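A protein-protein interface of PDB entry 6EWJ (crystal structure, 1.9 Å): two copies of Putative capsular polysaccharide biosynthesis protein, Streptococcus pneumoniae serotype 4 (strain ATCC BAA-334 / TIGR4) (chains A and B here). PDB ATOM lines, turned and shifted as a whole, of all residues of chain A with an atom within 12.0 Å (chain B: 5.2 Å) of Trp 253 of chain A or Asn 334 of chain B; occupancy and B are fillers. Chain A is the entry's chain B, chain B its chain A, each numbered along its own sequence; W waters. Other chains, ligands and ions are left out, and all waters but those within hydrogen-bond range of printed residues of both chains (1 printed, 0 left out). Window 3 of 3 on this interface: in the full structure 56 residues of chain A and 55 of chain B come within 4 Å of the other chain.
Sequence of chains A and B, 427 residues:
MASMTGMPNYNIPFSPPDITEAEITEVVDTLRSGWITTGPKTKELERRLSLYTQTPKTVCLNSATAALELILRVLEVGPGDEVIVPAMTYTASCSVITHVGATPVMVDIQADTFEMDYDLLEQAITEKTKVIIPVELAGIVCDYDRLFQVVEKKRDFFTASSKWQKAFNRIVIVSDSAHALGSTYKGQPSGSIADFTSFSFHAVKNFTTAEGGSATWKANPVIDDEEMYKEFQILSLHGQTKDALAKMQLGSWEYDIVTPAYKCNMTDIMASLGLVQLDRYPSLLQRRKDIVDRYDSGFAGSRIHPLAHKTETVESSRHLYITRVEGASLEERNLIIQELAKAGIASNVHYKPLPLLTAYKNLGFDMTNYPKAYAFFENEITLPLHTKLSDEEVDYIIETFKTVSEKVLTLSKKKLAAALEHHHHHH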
ATOM      1  N   GLN A 240      10.823  29.356  32.154  1.00  0.00           N
ATOM      2  CA  GLN A 240      12.259  29.291  31.949  1.00  0.00           C
ATOM      3  C   GLN A 240      12.926  30.201  32.963  1.00  0.00           C
ATOM      4  O   GLN A 240      12.452  31.325  33.180  1.00  0.00           O
ATOM      5  CB  GLN A 240      12.658  29.648  30.517  1.00  0.00           C
ATOM      6  CG  GLN A 240      14.140  29.470  30.213  1.00  0.00           C
ATOM      7  CD  GLN A 240      14.537  29.559  28.719  1.00  0.00           C
ATOM      8  OE1 GLN A 240      14.092  28.772  27.898  1.00  0.00           O
ATOM      9  NE2 GLN A 240      15.435  30.467  28.398  1.00  0.00           N
ATOM     10  N   THR A 241      13.984  29.697  33.593  1.00  0.00           N
ATOM     11  CA  THR A 241      14.858  30.478  34.472  1.00  0.00           C
ATOM     12  C   THR A 241      16.354  30.179  34.161  1.00  0.00           C
ATOM     13  O   THR A 241      16.681  29.121  33.626  1.00  0.00           O
ATOM     14  CB  THR A 241      14.626  30.116  35.954  1.00  0.00           C
ATOM     15  OG1 THR A 241      15.024  28.766  36.185  1.00  0.00           O
ATOM     16  CG2 THR A 241      13.161  30.274  36.362  1.00  0.00           C
ATOM     17  N   LYS A 242      17.237  31.122  34.494  1.00  0.00           N
ATOM     18  CA  LYS A 242      18.713  30.963  34.410  1.00  0.00           C
ATOM     19  C   LYS A 242      19.350  31.448  35.707  1.00  0.00           C
ATOM     20  O   LYS A 242      18.836  32.382  36.329  1.00  0.00           O
ATOM     21  CB  LYS A 242      19.314  31.798  33.274  1.00  0.00           C
ATOM     22  CG  LYS A 242      18.830  31.462  31.893  1.00  0.00           C
ATOM     23  CD  LYS A 242      19.926  31.723  30.882  1.00  0.00           C
ATOM     24  CE  LYS A 242      19.362  31.509  29.517  1.00  0.00           C
ATOM     25  NZ  LYS A 242      19.972  30.502  28.624  1.00  0.00           N
ATOM     26  N   ASP A 243      20.439  30.821  36.138  1.00  0.00           N
ATOM     27  CA  ASP A 243      21.157  31.320  37.342  1.00  0.00           C
ATOM     28  C   ASP A 243      22.154  32.478  37.087  1.00  0.00           C
ATOM     29  O   ASP A 243      22.259  33.052  35.985  1.00  0.00           O
ATOM     30  CB  ASP A 243      21.822  30.176  38.115  1.00  0.00           C
ATOM     31  CG  ASP A 243      22.829  29.375  37.282  1.00  0.00           C
ATOM     32  OD1 ASP A 243      23.408  29.905  36.314  1.00  0.00           O
ATOM     33  OD2 ASP A 243      23.039  28.187  37.629  1.00  0.00           O
ATOM     34  N   SER A 252      26.715  30.655  28.103  1.00  0.00           N
ATOM     35  CA  SER A 252      25.442  30.896  28.816  1.00  0.00           C
ATOM     36  C   SER A 252      24.266  30.173  28.171  1.00  0.00           C
ATOM     37  O   SER A 252      23.158  30.737  27.996  1.00  0.00           O
ATOM     38  CB  SER A 252      25.117  32.385  28.907  1.00  0.00           C
ATOM     39  OG  SER A 252      26.055  33.076  29.700  1.00  0.00           O
ATOM     40  N   TRP A 253      24.517  28.920  27.820  1.00  0.00           N
ATOM     41  CA  TRP A 253      23.494  28.061  27.218  1.00  0.00           C
ATOM     42  C   TRP A 253      22.468  27.567  28.269  1.00  0.00           C
ATOM     43  O   TRP A 253      21.306  27.408  27.966  1.00  0.00           O
ATOM     44  CB  TRP A 253      24.139  26.864  26.475  1.00  0.00           C
ATOM     45  CG  TRP A 253      24.880  25.929  27.359  1.00  0.00           C
ATOM     46  CD1 TRP A 253      26.194  26.015  27.715  1.00  0.00           C
ATOM     47  CD2 TRP A 253      24.360  24.784  28.043  1.00  0.00           C
ATOM     48  NE1 TRP A 253      26.529  25.010  28.576  1.00  0.00           N
ATOM     49  CE2 TRP A 253      25.425  24.237  28.802  1.00  0.00           C
ATOM     50  CE3 TRP A 253      23.095  24.188  28.119  1.00  0.00           C
ATOM     51  CZ2 TRP A 253      25.268  23.125  29.615  1.00  0.00           C
ATOM     52  CZ3 TRP A 253      22.948  23.056  28.910  1.00  0.00           C
ATOM     53  CH2 TRP A 253      24.023  22.542  29.651  1.00  0.00           C
ATOM     54  N   GLU A 254      22.894  27.341  29.509  1.00  0.00           N
ATOM     55  CA  GLU A 254      22.065  26.597  30.454  1.00  0.00           C
ATOM     56  C   GLU A 254      20.836  27.358  31.019  1.00  0.00           C
ATOM     57  O   GLU A 254      20.932  28.514  31.422  1.00  0.00           O
ATOM     58  CB  GLU A 254      22.939  26.010  31.564  1.00  0.00           C
ATOM     59  CG  GLU A 254      22.254  24.854  32.194  1.00  0.00           C
ATOM     60  CD  GLU A 254      23.052  24.168  33.240  1.00  0.00           C
ATOM     61  OE1 GLU A 254      24.258  24.465  33.371  1.00  0.00           O
ATOM     62  OE2 GLU A 254      22.444  23.307  33.912  1.00  0.00           O
ATOM     63  N   TYR A 255      19.688  26.677  31.030  1.00  0.00           N
ATOM     64  CA  TYR A 255      18.455  27.151  31.685  1.00  0.00           C
ATOM     65  C   TYR A 255      17.783  25.952  32.274  1.00  0.00           C
ATOM     66  O   TYR A 255      18.107  24.812  31.929  1.00  0.00           O
ATOM     67  CB  TYR A 255      17.494  27.858  30.728  1.00  0.00           C
ATOM     68  CG  TYR A 255      16.994  27.032  29.586  1.00  0.00           C
ATOM     69  CD1 TYR A 255      15.895  26.163  29.755  1.00  0.00           C
ATOM     70  CD2 TYR A 255      17.575  27.132  28.310  1.00  0.00           C
ATOM     71  CE1 TYR A 255      15.393  25.437  28.689  1.00  0.00           C
ATOM     72  CE2 TYR A 255      17.080  26.398  27.237  1.00  0.00           C
ATOM     73  CZ  TYR A 255      15.999  25.550  27.427  1.00  0.00           C
ATOM     74  OH  TYR A 255      15.462  24.822  26.385  1.00  0.00           O
ATOM     75  N   ASP A 256      16.812  26.226  33.133  1.00  0.00           N
ATOM     76  CA  ASP A 256      15.928  25.224  33.669  1.00  0.00           C
ATOM     77  C   ASP A 256      14.479  25.643  33.306  1.00  0.00           C
ATOM     78  O   ASP A 256      14.219  26.780  32.950  1.00  0.00           O
ATOM     79  CB  ASP A 256      16.121  25.137  35.169  1.00  0.00           C
ATOM     80  CG  ASP A 256      15.407  23.974  35.803  1.00  0.00           C
ATOM     81  OD1 ASP A 256      14.941  23.025  35.120  1.00  0.00           O
ATOM     82  OD2 ASP A 256      15.384  23.962  37.068  1.00  0.00           O
ATOM     83  N   ILE A 257      13.558  24.701  33.389  1.00  0.00           N
ATOM     84  CA  ILE A 257      12.126  24.968  33.242  1.00  0.00           C
ATOM     85  C   ILE A 257      11.515  24.580  34.578  1.00  0.00           C
ATOM     86  O   ILE A 257      11.642  23.443  34.985  1.00  0.00           O
ATOM     87  CB  ILE A 257      11.532  24.119  32.106  1.00  0.00           C
ATOM     88  CG1 ILE A 257      12.217  24.482  30.790  1.00  0.00           C
ATOM     89  CG2 ILE A 257      10.016  24.245  32.041  1.00  0.00           C
ATOM     90  CD1 ILE A 257      12.024  25.909  30.319  1.00  0.00           C
ATOM     91  N   SER B 329      33.056  14.218  26.976  1.00  0.00           N
ATOM     92  CA  SER B 329      32.161  14.145  28.137  1.00  0.00           C
ATOM     93  C   SER B 329      31.324  15.410  28.267  1.00  0.00           C
ATOM     94  O   SER B 329      31.597  16.425  27.645  1.00  0.00           O
ATOM     95  CB  SER B 329      32.961  13.952  29.431  1.00  0.00           C
ATOM     96  OG  SER B 329      33.675  15.135  29.784  1.00  0.00           O
ATOM     97  N   LEU B 330      30.325  15.333  29.140  1.00  0.00           N
ATOM     98  CA  LEU B 330      29.558  16.498  29.570  1.00  0.00           C
ATOM     99  C   LEU B 330      30.430  17.698  29.917  1.00  0.00           C
ATOM    100  O   LEU B 330      30.217  18.800  29.401  1.00  0.00           O
ATOM    101  CB  LEU B 330      28.688  16.157  30.794  1.00  0.00           C
ATOM    102  CG  LEU B 330      27.742  17.283  31.256  1.00  0.00           C
ATOM    103  CD1 LEU B 330      26.789  17.671  30.135  1.00  0.00           C
ATOM    104  CD2 LEU B 330      26.961  16.842  32.471  1.00  0.00           C
ATOM    105  N   GLU B 331      31.423  17.470  30.766  1.00  0.00           N
ATOM    106  CA  GLU B 331      32.268  18.526  31.265  1.00  0.00           C
ATOM    107  C   GLU B 331      33.122  19.119  30.160  1.00  0.00           C
ATOM    108  O   GLU B 331      33.335  20.345  30.072  1.00  0.00           O
ATOM    109  CB  GLU B 331      33.085  17.992  32.447  1.00  0.00           C
ATOM    110  CG  GLU B 331      34.100  19.002  32.956  1.00  0.00           C
ATOM    111  CD  GLU B 331      34.708  18.623  34.290  1.00  0.00           C
ATOM    112  OE1 GLU B 331      34.586  17.428  34.699  1.00  0.00           O
ATOM    113  OE2 GLU B 331      35.341  19.526  34.888  1.00  0.00           O
ATOM    114  N   GLU B 332      33.568  18.253  29.271  1.00  0.00           N
ATOM    115  CA  GLU B 332      34.416  18.673  28.151  1.00  0.00           C
ATOM    116  C   GLU B 332      33.598  19.455  27.140  1.00  0.00           C
ATOM    117  O   GLU B 332      34.064  20.465  26.615  1.00  0.00           O
ATOM    118  CB  GLU B 332      35.109  17.465  27.512  1.00  0.00           C
ATOM    119  CG  GLU B 332      36.166  16.835  28.402  1.00  0.00           C
ATOM    120  CD  GLU B 332      36.637  15.474  27.897  1.00  0.00           C
ATOM    121  OE1 GLU B 332      35.862  14.788  27.192  1.00  0.00           O
ATOM    122  OE2 GLU B 332      37.772  15.098  28.193  1.00  0.00           O
ATOM    123  N   ARG B 333      32.371  19.012  26.881  1.00  0.00           N
ATOM    124  CA  ARG B 333      31.444  19.782  26.011  1.00  0.00           C
ATOM    125  C   ARG B 333      31.261  21.178  26.549  1.00  0.00           C
ATOM    126  O   ARG B 333      31.297  22.170  25.791  1.00  0.00           O
ATOM    127  CB  ARG B 333      30.069  19.109  25.870  1.00  0.00           C
ATOM    128  CG  ARG B 333      29.165  19.731  24.757  1.00  0.00           C
ATOM    129  CD  ARG B 333      28.366  20.965  25.170  1.00  0.00           C
ATOM    130  NE  ARG B 333      27.651  20.702  26.410  1.00  0.00           N
ATOM    131  CZ  ARG B 333      26.531  20.007  26.502  1.00  0.00           C
ATOM    132  NH1 ARG B 333      25.916  19.526  25.436  1.00  0.00           N
ATOM    133  NH2 ARG B 333      26.002  19.830  27.703  1.00  0.00           N
ATOM    134  N   ASN B 334      31.020  21.290  27.850  1.00  0.00           N
ATOM    135  CA  ASN B 334      30.737  22.608  28.433  1.00  0.00           C
ATOM    136  C   ASN B 334      31.968  23.498  28.284  1.00  0.00           C
ATOM    137  O   ASN B 334      31.815  24.655  27.935  1.00  0.00           O
ATOM    138  CB  ASN B 334      30.270  22.498  29.893  1.00  0.00           C
ATOM    139  CG  ASN B 334      28.956  21.726  30.049  1.00  0.00           C
ATOM    140  OD1 ASN B 334      28.185  21.521  29.102  1.00  0.00           O
ATOM    141  ND2 ASN B 334      28.686  21.298  31.304  1.00  0.00           N
ATOM    142  N   LEU B 335      33.167  22.935  28.515  1.00  0.00           N
ATOM    143  CA  LEU B 335      34.429  23.692  28.355  1.00  0.00           C
ATOM    144  C   LEU B 335      34.592  24.175  26.922  1.00  0.00           C
ATOM    145  O   LEU B 335      34.844  25.363  26.704  1.00  0.00           O
ATOM    146  CB  LEU B 335      35.665  22.891  28.806  1.00  0.00           C
ATOM    147  CG  LEU B 335      37.044  23.593  28.722  1.00  0.00           C
ATOM    148  CD1 LEU B 335      37.051  25.004  29.342  1.00  0.00           C
ATOM    149  CD2 LEU B 335      38.124  22.752  29.361  1.00  0.00           C
ATOM    150  N   ILE B 336      34.324  23.296  25.949  1.00  0.00           N
ATOM    151  CA  ILE B 336      34.366  23.686  24.514  1.00  0.00           C
ATOM    152  C   ILE B 336      33.429  24.888  24.200  1.00  0.00           C
ATOM    153  O   ILE B 336      33.821  25.827  23.507  1.00  0.00           O
ATOM    154  CB  ILE B 336      34.077  22.487  23.573  1.00  0.00           C
ATOM    155  CG1 ILE B 336      35.222  21.463  23.644  1.00  0.00           C
ATOM    156  CG2 ILE B 336      33.924  22.957  22.118  1.00  0.00           C
ATOM    157  CD1 ILE B 336      34.910  20.102  23.039  1.00  0.00           C
ATOM    158  N   ILE B 337      32.222  24.893  24.746  1.00  0.00           N
ATOM    159  CA  ILE B 337      31.321  26.030  24.543  1.00  0.00           C
ATOM    160  C   ILE B 337      31.913  27.323  25.099  1.00  0.00           C
ATOM    161  O   ILE B 337      31.900  28.356  24.429  1.00  0.00           O
ATOM    162  CB  ILE B 337      29.938  25.788  25.140  1.00  0.00           C
ATOM    163  CG1 ILE B 337      29.193  24.809  24.239  1.00  0.00           C
ATOM    164  CG2 ILE B 337      29.145  27.089  25.277  1.00  0.00           C
ATOM    165  CD1 ILE B 337      27.910  24.317  24.848  1.00  0.00           C
ATOM    166  N   GLN B 338      32.453  27.269  26.304  1.00  0.00           N
ATOM    167  CA  GLN B 338      33.088  28.473  26.891  1.00  0.00           C
ATOM    168  C   GLN B 338      34.341  28.938  26.094  1.00  0.00           C
ATOM    169  O   GLN B 338      34.587  30.152  25.969  1.00  0.00           O
ATOM    170  CB  GLN B 338      33.393  28.270  28.388  1.00  0.00           C
ATOM    171  CG  GLN B 338      32.184  27.951  29.264  1.00  0.00           C
ATOM    172  CD  GLN B 338      31.098  29.006  29.291  1.00  0.00           C
ATOM    173  OE1 GLN B 338      31.331  30.204  29.055  1.00  0.00           O
ATOM    174  NE2 GLN B 338      29.873  28.562  29.619  1.00  0.00           N
ATOM    175  N   SER B 347      27.233  29.819  20.736  1.00  0.00           N
ATOM    176  CA  SER B 347      26.866  28.434  20.475  1.00  0.00           C
ATOM    177  C   SER B 347      25.750  28.102  21.437  1.00  0.00           C
ATOM    178  O   SER B 347      25.445  28.906  22.365  1.00  0.00           O
ATOM    179  CB  SER B 347      28.076  27.492  20.596  1.00  0.00           C
ATOM    180  OG  SER B 347      28.598  27.390  21.922  1.00  0.00           O
ATOM    181  N   ASN B 348      25.109  26.967  21.220  1.00  0.00           N
ATOM    182  CA  ASN B 348      23.982  26.611  22.000  1.00  0.00           C
ATOM    183  C   ASN B 348      23.875  25.142  22.104  1.00  0.00           C
ATOM    184  O   ASN B 348      24.701  24.410  21.539  1.00  0.00           O
ATOM    185  CB  ASN B 348      22.736  27.207  21.342  1.00  0.00           C
ATOM    186  CG  ASN B 348      21.689  27.621  22.331  1.00  0.00           C
ATOM    187  OD1 ASN B 348      21.642  27.143  23.481  1.00  0.00           O
ATOM    188  ND2 ASN B 348      20.795  28.486  21.881  1.00  0.00           N
ATOM    189  N   VAL B 349      22.902  24.690  22.887  1.00  0.00           N
ATOM    190  CA  VAL B 349      22.688  23.269  23.117  1.00  0.00           C
ATOM    191  C   VAL B 349      21.225  22.985  22.877  1.00  0.00           C
ATOM    192  O   VAL B 349      20.348  23.624  23.475  1.00  0.00           O
ATOM    193  CB  VAL B 349      23.122  22.774  24.538  1.00  0.00           C
ATOM    194  CG1 VAL B 349      22.714  21.313  24.751  1.00  0.00           C
ATOM    195  CG2 VAL B 349      24.601  22.941  24.742  1.00  0.00           C
ATOM    196  N   LYS B 352      18.786  19.902  26.454  1.00  0.00           N
ATOM    197  CA  LYS B 352      18.651  19.134  27.657  1.00  0.00           C
ATOM    198  C   LYS B 352      17.450  18.247  27.465  1.00  0.00           C
ATOM    199  O   LYS B 352      16.424  18.734  27.057  1.00  0.00           O
ATOM    200  CB  LYS B 352      18.335  20.045  28.842  1.00  0.00           C
ATOM    201  CG  LYS B 352      19.499  20.826  29.325  1.00  0.00           C
ATOM    202  CD  LYS B 352      19.184  21.393  30.717  1.00  0.00           C
ATOM    203  CE  LYS B 352      20.409  21.999  31.308  1.00  0.00           C
ATOM    204  NZ  LYS B 352      20.087  22.719  32.587  1.00  0.00           N
ATOM    205  N   PHE B 377      22.505  14.594  24.005  1.00  0.00           N
ATOM    206  CA  PHE B 377      22.711  15.874  24.705  1.00  0.00           C
ATOM    207  C   PHE B 377      24.118  16.089  25.190  1.00  0.00           C
ATOM    208  O   PHE B 377      24.698  17.160  25.011  1.00  0.00           O
ATOM    209  CB  PHE B 377      21.759  15.969  25.894  1.00  0.00           C
ATOM    210  CG  PHE B 377      22.224  16.896  26.988  1.00  0.00           C
ATOM    211  CD1 PHE B 377      22.208  18.296  26.807  1.00  0.00           C
ATOM    212  CD2 PHE B 377      22.655  16.389  28.224  1.00  0.00           C
ATOM    213  CE1 PHE B 377      22.676  19.152  27.797  1.00  0.00           C
ATOM    214  CE2 PHE B 377      23.113  17.251  29.198  1.00  0.00           C
ATOM    215  CZ  PHE B 377      23.100  18.639  28.992  1.00  0.00           C
HETATM  216  O   HOH W   1      17.646  22.702  26.578  1.00  0.00           O
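OE2 of Glu 254 of chain A is in salt-bridge range of NZ of Lys 352 of chain B (2.8 Å). The side-chain amino group of Lys 352 of chain B is in hydrogen-bond range of the backbone carbonyl oxygen of Tyr 255 of chain A (3.0 Å).
O of Leu 330 of chain B lies close to OD1 of Asn 334 of chain B. The guanidinium group of Arg 333 of chain B lies within hydrogen-bond range of the side-chain amide oxygen of Asn 334 of chain B, at 2.9 Å. NH1 of Arg 333 of chain B sits at hydrogen-bond distance from O of Phe 377 of chain B. The side-chain amino group (NZ) of Lys 242 of chain A sits at hydrogen-bond distance from the backbone carbonyl oxygen (O) of Trp 253 of chain A (3.4 Å).
Among the printed residues, pairs that only touch across the chains: Trp 253 of chain A with Asn 334 of chain B (3.4 Å), Trp 253 of chain A with Lys 352 of chain B (3.6 Å), Trp 253 of chain A with Ile 337 of chain B (3.7 Å), Trp 253 of chain A with Val 349 of chain B (3.8 Å), Trp 253 of chain A with Arg 333 of chain B (3.9 Å) and Trp 253 of chain A with Asn 348 of chain B (3.9 Å).
Trp 253 of chain A touches just these residues of chain B: Arg 333 (3.9 Å), Asn 334 (3.4 Å), Ile 337 (3.7 Å), Asn 348 (3.9 Å), Val 349 (3.8 Å) and Lys 352 (3.6 Å). Asn 334 of chain B touches one residue of chain A. No residue of chain A comes within 4 Å of Ser 329 of chain B. No residue of chain A comes within 4 Å of Leu 330 of chain B. No residue of chain A comes within 4 Å of Glu 331 of chain B. No residue of chain A comes within 4 Å of Leu 335 of chain B. No residue of chain A comes within 4 Å of Gln 338 of chain B. No residue of chain A comes within 4 Å of Ser 347 of chain B. Asn 348 of chain B touches just one residue of chain A: Trp 253. Of the printed residues of chain B, Glu 254 of chain A touches Lys 352. Of the printed residues of chain B, Tyr 255 of chain A touches Lys 352 (3.0 Å). Of the printed residues of chain A, Lys 352 of chain B touches Trp 253, Glu 254 and Tyr 255. The nearest residue of chain B that does not touch Trp 253 of chain A is Phe 377 of chain B (4.1 Å).
Hydrophobic or aromatic side chains of chain A that line the printed part of chain B: Trp 253. Among the printed residues, Asp or Glu carboxylates within 4 Å of a Lys or Arg side-chain nitrogen of the other chain: Glu 254 of chain A with Lys 352 of chain B.
No position is printed for both chains.
Water W1 lies within hydrogen-bond range of the backbone NH of Lys 352 of chain B (3.0 Å) and the side-chain hydroxyl of Tyr 255 of chain A (3.0 Å).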
